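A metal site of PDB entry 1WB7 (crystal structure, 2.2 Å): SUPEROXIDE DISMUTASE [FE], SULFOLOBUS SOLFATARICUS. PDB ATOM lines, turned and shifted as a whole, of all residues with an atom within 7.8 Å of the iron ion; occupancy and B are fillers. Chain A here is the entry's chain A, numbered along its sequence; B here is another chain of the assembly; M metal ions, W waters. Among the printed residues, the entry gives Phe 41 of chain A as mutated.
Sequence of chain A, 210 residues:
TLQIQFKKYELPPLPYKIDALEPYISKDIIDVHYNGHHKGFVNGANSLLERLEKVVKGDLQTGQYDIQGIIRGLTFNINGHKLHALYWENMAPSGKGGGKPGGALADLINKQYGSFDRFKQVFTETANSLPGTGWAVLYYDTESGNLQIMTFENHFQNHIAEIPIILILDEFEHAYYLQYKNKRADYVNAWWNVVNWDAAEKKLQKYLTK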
ATOM      1  N   HIS A  33      -1.072  -0.131   6.639  1.00  0.00           N
ATOM      2  CA  HIS A  33      -2.089   0.503   7.459  1.00  0.00           C
ATOM      3  C   HIS A  33      -1.728   0.390   8.945  1.00  0.00           C
ATOM      4  O   HIS A  33      -1.906   1.325   9.713  1.00  0.00           O
ATOM      5  CB  HIS A  33      -3.442  -0.141   7.191  1.00  0.00           C
ATOM      6  CG  HIS A  33      -4.608   0.709   7.588  1.00  0.00           C
ATOM      7  ND1 HIS A  33      -5.907   0.378   7.273  1.00  0.00           N
ATOM      8  CD2 HIS A  33      -4.673   1.874   8.269  1.00  0.00           C
ATOM      9  CE1 HIS A  33      -6.724   1.316   7.732  1.00  0.00           C
ATOM     10  NE2 HIS A  33      -5.998   2.229   8.341  1.00  0.00           N
ATOM     11  N   TYR A  34      -1.208  -0.767   9.329  1.00  0.00           N
ATOM     12  CA  TYR A  34      -0.823  -1.020  10.719  1.00  0.00           C
ATOM     13  C   TYR A  34       0.615  -0.553  11.001  1.00  0.00           C
ATOM     14  O   TYR A  34       0.842   0.292  11.883  1.00  0.00           O
ATOM     15  CB  TYR A  34      -0.945  -2.514  11.029  1.00  0.00           C
ATOM     16  CG  TYR A  34      -0.428  -2.923  12.392  1.00  0.00           C
ATOM     17  CD1 TYR A  34      -1.126  -2.568  13.549  1.00  0.00           C
ATOM     18  CD2 TYR A  34       0.758  -3.635  12.531  1.00  0.00           C
ATOM     19  CE1 TYR A  34      -0.653  -2.901  14.810  1.00  0.00           C
ATOM     20  CE2 TYR A  34       1.242  -3.975  13.788  1.00  0.00           C
ATOM     21  CZ  TYR A  34       0.527  -3.609  14.925  1.00  0.00           C
ATOM     22  OH  TYR A  34       1.003  -3.943  16.173  1.00  0.00           O
ATOM     23  N   HIS A  37       0.692   3.631   9.024  1.00  0.00           N
ATOM     24  CA  HIS A  37      -0.250   4.600   9.561  1.00  0.00           C
ATOM     25  C   HIS A  37      -0.478   4.552  11.073  1.00  0.00           C
ATOM     26  O   HIS A  37      -0.283   5.552  11.765  1.00  0.00           O
ATOM     27  CB  HIS A  37      -1.583   4.479   8.820  1.00  0.00           C
ATOM     28  CG  HIS A  37      -1.505   4.869   7.379  1.00  0.00           C
ATOM     29  ND1 HIS A  37      -1.488   6.193   6.966  1.00  0.00           N
ATOM     30  CD2 HIS A  37      -1.407   4.124   6.255  1.00  0.00           C
ATOM     31  CE1 HIS A  37      -1.377   6.239   5.652  1.00  0.00           C
ATOM     32  NE2 HIS A  37      -1.326   4.996   5.197  1.00  0.00           N
ATOM     33  N   HIS A  38      -0.886   3.399  11.597  1.00  0.00           N
ATOM     34  CA  HIS A  38      -1.136   3.309  13.041  1.00  0.00           C
ATOM     35  C   HIS A  38       0.121   3.622  13.863  1.00  0.00           C
ATOM     36  O   HIS A  38       0.071   4.401  14.808  1.00  0.00           O
ATOM     37  CB  HIS A  38      -1.671   1.916  13.409  1.00  0.00           C
ATOM     38  CG  HIS A  38      -2.230   1.835  14.802  1.00  0.00           C
ATOM     39  ND1 HIS A  38      -2.956   0.753  15.248  1.00  0.00           N
ATOM     40  CD2 HIS A  38      -2.155   2.701  15.844  1.00  0.00           C
ATOM     41  CE1 HIS A  38      -3.313   0.955  16.507  1.00  0.00           C
ATOM     42  NE2 HIS A  38      -2.837   2.126  16.892  1.00  0.00           N
ATOM     43  N   PHE A  41       0.805   7.226  14.274  1.00  0.00           N
ATOM     44  CA  PHE A  41      -0.018   7.950  15.245  1.00  0.00           C
ATOM     45  C   PHE A  41       0.507   7.801  16.655  1.00  0.00           C
ATOM     46  O   PHE A  41       0.512   8.757  17.428  1.00  0.00           O
ATOM     47  CB  PHE A  41      -1.463   7.469  15.180  1.00  0.00           C
ATOM     48  CG  PHE A  41      -2.147   7.799  13.898  1.00  0.00           C
ATOM     49  CD1 PHE A  41      -2.254   9.127  13.485  1.00  0.00           C
ATOM     50  CD2 PHE A  41      -2.628   6.797  13.066  1.00  0.00           C
ATOM     51  CE1 PHE A  41      -2.834   9.447  12.250  1.00  0.00           C
ATOM     52  CE2 PHE A  41      -3.210   7.110  11.839  1.00  0.00           C
ATOM     53  CZ  PHE A  41      -3.318   8.432  11.433  1.00  0.00           C
ATOM     54  N   GLY A  80      -6.132   9.088  16.275  1.00  0.00           N
ATOM     55  CA  GLY A  80      -5.614   8.270  15.187  1.00  0.00           C
ATOM     56  C   GLY A  80      -5.226   6.908  15.733  1.00  0.00           C
ATOM     57  O   GLY A  80      -5.523   5.872  15.143  1.00  0.00           O
ATOM     58  N   LEU A  83      -8.633   5.059  17.534  1.00  0.00           N
ATOM     59  CA  LEU A  83      -9.576   4.566  16.540  1.00  0.00           C
ATOM     60  C   LEU A  83      -9.037   3.377  15.730  1.00  0.00           C
ATOM     61  O   LEU A  83      -9.790   2.455  15.420  1.00  0.00           O
ATOM     62  CB  LEU A  83      -9.989   5.707  15.600  1.00  0.00           C
ATOM     63  CG  LEU A  83     -10.763   6.834  16.292  1.00  0.00           C
ATOM     64  CD1 LEU A  83     -11.198   7.869  15.265  1.00  0.00           C
ATOM     65  CD2 LEU A  83     -11.981   6.254  17.026  1.00  0.00           C
ATOM     66  N   HIS A  84      -7.764   3.398  15.379  1.00  0.00           N
ATOM     67  CA  HIS A  84      -7.206   2.280  14.636  1.00  0.00           C
ATOM     68  C   HIS A  84      -7.167   1.051  15.537  1.00  0.00           C
ATOM     69  O   HIS A  84      -7.428  -0.072  15.091  1.00  0.00           O
ATOM     70  CB  HIS A  84      -5.814   2.609  14.094  1.00  0.00           C
ATOM     71  CG  HIS A  84      -5.846   3.460  12.865  1.00  0.00           C
ATOM     72  ND1 HIS A  84      -6.016   4.821  12.894  1.00  0.00           N
ATOM     73  CD2 HIS A  84      -5.772   3.133  11.547  1.00  0.00           C
ATOM     74  CE1 HIS A  84      -6.045   5.296  11.663  1.00  0.00           C
ATOM     75  NE2 HIS A  84      -5.897   4.290  10.826  1.00  0.00           N
ATOM     76  N   TYR A  87     -10.439  -0.305  15.469  1.00  0.00           N
ATOM     77  CA  TYR A  87     -10.663  -0.825  14.134  1.00  0.00           C
ATOM     78  C   TYR A  87     -10.148  -2.255  13.972  1.00  0.00           C
ATOM     79  O   TYR A  87     -10.873  -3.118  13.476  1.00  0.00           O
ATOM     80  CB  TYR A  87      -9.983   0.116  13.132  1.00  0.00           C
ATOM     81  CG  TYR A  87     -10.142  -0.273  11.683  1.00  0.00           C
ATOM     82  CD1 TYR A  87     -11.396  -0.392  11.091  1.00  0.00           C
ATOM     83  CD2 TYR A  87      -9.014  -0.451  10.872  1.00  0.00           C
ATOM     84  CE1 TYR A  87     -11.534  -0.659   9.728  1.00  0.00           C
ATOM     85  CE2 TYR A  87      -9.131  -0.730   9.514  1.00  0.00           C
ATOM     86  CZ  TYR A  87     -10.393  -0.834   8.949  1.00  0.00           C
ATOM     87  OH  TYR A  87     -10.497  -1.069   7.606  1.00  0.00           O
ATOM     88  N   TRP A  88      -8.897  -2.505  14.364  1.00  0.00           N
ATOM     89  CA  TRP A  88      -8.306  -3.841  14.243  1.00  0.00           C
ATOM     90  C   TRP A  88      -9.102  -4.884  15.027  1.00  0.00           C
ATOM     91  O   TRP A  88      -9.364  -5.976  14.527  1.00  0.00           O
ATOM     92  CB  TRP A  88      -6.860  -3.854  14.770  1.00  0.00           C
ATOM     93  CG  TRP A  88      -5.977  -2.836  14.153  1.00  0.00           C
ATOM     94  CD1 TRP A  88      -5.124  -1.988  14.818  1.00  0.00           C
ATOM     95  CD2 TRP A  88      -5.853  -2.524  12.770  1.00  0.00           C
ATOM     96  NE1 TRP A  88      -4.489  -1.171  13.928  1.00  0.00           N
ATOM     97  CE2 TRP A  88      -4.911  -1.474  12.653  1.00  0.00           C
ATOM     98  CE3 TRP A  88      -6.445  -3.032  11.597  1.00  0.00           C
ATOM     99  CZ2 TRP A  88      -4.556  -0.914  11.420  1.00  0.00           C
ATOM    100  CZ3 TRP A  88      -6.092  -2.465  10.371  1.00  0.00           C
ATOM    101  CH2 TRP A  88      -5.149  -1.426  10.297  1.00  0.00           C
ATOM    102  N   GLY A 134     -12.506   9.981   6.963  1.00  0.00           N
ATOM    103  CA  GLY A 134     -12.977   9.926   8.324  1.00  0.00           C
ATOM    104  C   GLY A 134     -13.375   8.517   8.726  1.00  0.00           C
ATOM    105  O   GLY A 134     -12.740   7.541   8.313  1.00  0.00           O
ATOM    106  N   TRP A 135     -14.434   8.415   9.523  1.00  0.00           N
ATOM    107  CA  TRP A 135     -14.918   7.135  10.029  1.00  0.00           C
ATOM    108  C   TRP A 135     -16.432   7.094  10.135  1.00  0.00           C
ATOM    109  O   TRP A 135     -17.111   8.117  10.135  1.00  0.00           O
ATOM    110  CB  TRP A 135     -14.373   6.867  11.442  1.00  0.00           C
ATOM    111  CG  TRP A 135     -12.904   6.986  11.589  1.00  0.00           C
ATOM    112  CD1 TRP A 135     -12.159   8.134  11.574  1.00  0.00           C
ATOM    113  CD2 TRP A 135     -11.972   5.909  11.768  1.00  0.00           C
ATOM    114  NE1 TRP A 135     -10.827   7.838  11.718  1.00  0.00           N
ATOM    115  CE2 TRP A 135     -10.680   6.478  11.836  1.00  0.00           C
ATOM    116  CE3 TRP A 135     -12.109   4.520  11.872  1.00  0.00           C
ATOM    117  CZ2 TRP A 135      -9.527   5.701  12.007  1.00  0.00           C
ATOM    118  CZ3 TRP A 135     -10.954   3.749  12.036  1.00  0.00           C
ATOM    119  CH2 TRP A 135      -9.684   4.345  12.098  1.00  0.00           C
ATOM    120  N   HIS A 155      -9.911  12.246  12.105  1.00  0.00           N
ATOM    121  CA  HIS A 155      -9.979  11.339  13.255  1.00  0.00           C
ATOM    122  C   HIS A 155     -10.646  11.943  14.494  1.00  0.00           C
ATOM    123  O   HIS A 155     -11.055  11.222  15.395  1.00  0.00           O
ATOM    124  CB  HIS A 155      -8.569  10.899  13.702  1.00  0.00           C
ATOM    125  CG  HIS A 155      -7.758  10.238  12.623  1.00  0.00           C
ATOM    126  ND1 HIS A 155      -8.183   9.116  11.949  1.00  0.00           N
ATOM    127  CD2 HIS A 155      -6.530  10.544  12.131  1.00  0.00           C
ATOM    128  CE1 HIS A 155      -7.244   8.743  11.097  1.00  0.00           C
ATOM    129  NE2 HIS A 155      -6.239   9.591  11.186  1.00  0.00           N
ATOM    130  N   ASP A 170     -13.186   2.379   9.186  1.00  0.00           N
ATOM    131  CA  ASP A 170     -12.219   3.388   8.749  1.00  0.00           C
ATOM    132  C   ASP A 170     -12.539   3.834   7.314  1.00  0.00           C
ATOM    133  O   ASP A 170     -12.616   3.005   6.401  1.00  0.00           O
ATOM    134  CB  ASP A 170     -10.797   2.814   8.791  1.00  0.00           C
ATOM    135  CG  ASP A 170      -9.735   3.868   8.505  1.00  0.00           C
ATOM    136  OD1 ASP A 170     -10.098   5.011   8.158  1.00  0.00           O
ATOM    137  OD2 ASP A 170      -8.541   3.546   8.633  1.00  0.00           O
ATOM    138  N   GLU A 171     -12.704   5.131   7.122  1.00  0.00           N
ATOM    139  CA  GLU A 171     -13.000   5.629   5.791  1.00  0.00           C
ATOM    140  C   GLU A 171     -11.941   6.562   5.206  1.00  0.00           C
ATOM    141  O   GLU A 171     -12.225   7.332   4.300  1.00  0.00           O
ATOM    142  CB  GLU A 171     -14.377   6.314   5.777  1.00  0.00           C
ATOM    143  CG  GLU A 171     -15.527   5.350   6.009  1.00  0.00           C
ATOM    144  CD  GLU A 171     -16.877   5.986   5.763  1.00  0.00           C
ATOM    145  OE1 GLU A 171     -17.183   6.302   4.592  1.00  0.00           O
ATOM    146  OE2 GLU A 171     -17.631   6.154   6.741  1.00  0.00           O
ATOM    147  N   PHE A 172     -10.727   6.497   5.732  1.00  0.00           N
ATOM    148  CA  PHE A 172      -9.638   7.291   5.160  1.00  0.00           C
ATOM    149  C   PHE A 172      -9.310   6.497   3.904  1.00  0.00           C
ATOM    150  O   PHE A 172      -9.541   5.297   3.853  1.00  0.00           O
ATOM    151  CB  PHE A 172      -8.419   7.324   6.076  1.00  0.00           C
ATOM    152  CG  PHE A 172      -8.346   8.561   6.938  1.00  0.00           C
ATOM    153  CD1 PHE A 172      -9.295   8.793   7.933  1.00  0.00           C
ATOM    154  CD2 PHE A 172      -7.326   9.491   6.750  1.00  0.00           C
ATOM    155  CE1 PHE A 172      -9.237   9.952   8.709  1.00  0.00           C
ATOM    156  CE2 PHE A 172      -7.268  10.650   7.526  1.00  0.00           C
ATOM    157  CZ  PHE A 172      -8.223  10.881   8.505  1.00  0.00           C
ATOM    158  N   GLU A 173      -8.777   7.164   2.889  1.00  0.00           N
ATOM    159  CA  GLU A 173      -8.483   6.468   1.648  1.00  0.00           C
ATOM    160  C   GLU A 173      -7.447   5.357   1.743  1.00  0.00           C
ATOM    161  O   GLU A 173      -7.519   4.384   0.998  1.00  0.00           O
ATOM    162  CB  GLU A 173      -8.074   7.491   0.586  1.00  0.00           C
ATOM    163  CG  GLU A 173      -9.192   8.491   0.310  1.00  0.00           C
ATOM    164  CD  GLU A 173      -8.797   9.576  -0.671  1.00  0.00           C
ATOM    165  OE1 GLU A 173      -7.754  10.223  -0.446  1.00  0.00           O
ATOM    166  OE2 GLU A 173      -9.536   9.773  -1.661  1.00  0.00           O
ATOM    167  N   HIS A 174      -6.499   5.478   2.685  1.00  0.00           N
ATOM    168  CA  HIS A 174      -5.466   4.457   2.848  1.00  0.00           C
ATOM    169  C   HIS A 174      -6.019   3.129   3.354  1.00  0.00           C
ATOM    170  O   HIS A 174      -5.319   2.124   3.387  1.00  0.00           O
ATOM    171  CB  HIS A 174      -4.368   4.938   3.799  1.00  0.00           C
ATOM    172  CG  HIS A 174      -4.835   5.184   5.204  1.00  0.00           C
ATOM    173  ND1 HIS A 174      -4.860   6.436   5.767  1.00  0.00           N
ATOM    174  CD2 HIS A 174      -5.303   4.333   6.142  1.00  0.00           C
ATOM    175  CE1 HIS A 174      -5.322   6.352   7.008  1.00  0.00           C
ATOM    176  NE2 HIS A 174      -5.594   5.084   7.257  1.00  0.00           N
ATOM    177  N   ALA A 175      -7.284   3.120   3.757  1.00  0.00           N
ATOM    178  CA  ALA A 175      -7.885   1.894   4.254  1.00  0.00           C
ATOM    179  C   ALA A 175      -8.390   1.018   3.113  1.00  0.00           C
ATOM    180  O   ALA A 175      -8.716  -0.143   3.329  1.00  0.00           O
ATOM    181  CB  ALA A 175      -9.026   2.229   5.192  1.00  0.00           C
ATOM    182  N   TYR A 176      -8.433   1.572   1.911  1.00  0.00           N
ATOM    183  CA  TYR A 176      -8.958   0.808   0.773  1.00  0.00           C
ATOM    184  C   TYR A 176      -8.394   1.139  -0.610  1.00  0.00           C
ATOM    185  O   TYR A 176      -8.545   0.347  -1.528  1.00  0.00           O
ATOM    186  CB  TYR A 176     -10.475   0.990   0.715  1.00  0.00           C
ATOM    187  CG  TYR A 176     -10.906   2.426   0.461  1.00  0.00           C
ATOM    188  CD1 TYR A 176     -10.841   2.990  -0.810  1.00  0.00           C
ATOM    189  CD2 TYR A 176     -11.345   3.241   1.517  1.00  0.00           C
ATOM    190  CE1 TYR A 176     -11.206   4.319  -1.044  1.00  0.00           C
ATOM    191  CE2 TYR A 176     -11.702   4.578   1.292  1.00  0.00           C
ATOM    192  CZ  TYR A 176     -11.632   5.106   0.016  1.00  0.00           C
ATOM    193  OH  TYR A 176     -11.980   6.423  -0.198  1.00  0.00           O
ATOM    194  N   TYR A 187     -15.695  -1.023  -0.930  1.00  0.00           N
ATOM    195  CA  TYR A 187     -14.916  -1.367   0.258  1.00  0.00           C
ATOM    196  C   TYR A 187     -15.875  -1.486   1.436  1.00  0.00           C
ATOM    197  O   TYR A 187     -15.765  -2.395   2.257  1.00  0.00           O
ATOM    198  CB  TYR A 187     -13.881  -0.270   0.523  1.00  0.00           C
ATOM    199  CG  TYR A 187     -13.452  -0.125   1.968  1.00  0.00           C
ATOM    200  CD1 TYR A 187     -12.681  -1.113   2.584  1.00  0.00           C
ATOM    201  CD2 TYR A 187     -13.806   0.994   2.715  1.00  0.00           C
ATOM    202  CE1 TYR A 187     -12.267  -0.970   3.916  1.00  0.00           C
ATOM    203  CE2 TYR A 187     -13.401   1.143   4.038  1.00  0.00           C
ATOM    204  CZ  TYR A 187     -12.626   0.155   4.640  1.00  0.00           C
ATOM    205  OH  TYR A 187     -12.228   0.302   5.947  1.00  0.00           O
ATOM    206  N   GLU B 173      -4.989  11.683   0.131  1.00  0.00           N
ATOM    207  CA  GLU B 173      -4.181  10.508  -0.151  1.00  0.00           C
ATOM    208  C   GLU B 173      -4.249  10.000  -1.587  1.00  0.00           C
ATOM    209  O   GLU B 173      -3.281   9.440  -2.089  1.00  0.00           O
ATOM    210  CB  GLU B 173      -4.535   9.399   0.841  1.00  0.00           C
ATOM    211  CG  GLU B 173      -4.263   9.816   2.279  1.00  0.00           C
ATOM    212  CD  GLU B 173      -4.679   8.781   3.289  1.00  0.00           C
ATOM    213  OE1 GLU B 173      -5.843   8.343   3.237  1.00  0.00           O
ATOM    214  OE2 GLU B 173      -3.832   8.405   4.146  1.00  0.00           O
HETATM  215 FE    FE M   1      -6.726   4.193   8.863  1.00  0.00          FE
HETATM  216  O   HOH W   1      -7.629   6.368   9.210  1.00  0.00           O
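The side-chain carboxylate of Asp 170 is in hydrogen-bond range of the backbone NH of Phe 172 (2.9 Å). The side-chain hydroxyl (OH) of Tyr 187 lies within hydrogen-bond range of the backbone carbonyl oxygen (O) of Asp 170 (2.8 Å). O of His 84 lies close to NE1 of Trp 88 (3.3 Å). A ring nitrogen (ND1) of His 84 sits at hydrogen-bond distance from the backbone carbonyl oxygen of Gly 80 (2.5 Å). The side-chain carboxylate (OE2) of Glu 173 of chain B lies within hydrogen-bond range of a ring nitrogen (ND1) of His 174, 2.7 Å away. O of His 33 sits at hydrogen-bond distance from N of His 38, at 3.0 Å.
Within 4 Å of the iron ion: His 33, His 84, Asp 170 and His 174. The nearest printed residue that does not touch the iron ion is Trp 135 (4.4 Å).
The iron ion is bound by OD2 of Asp 170, NE2 of His 84, NE2 of His 174, NE2 of His 33 and water W1. The iron ion has five donor atoms within binding distance.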
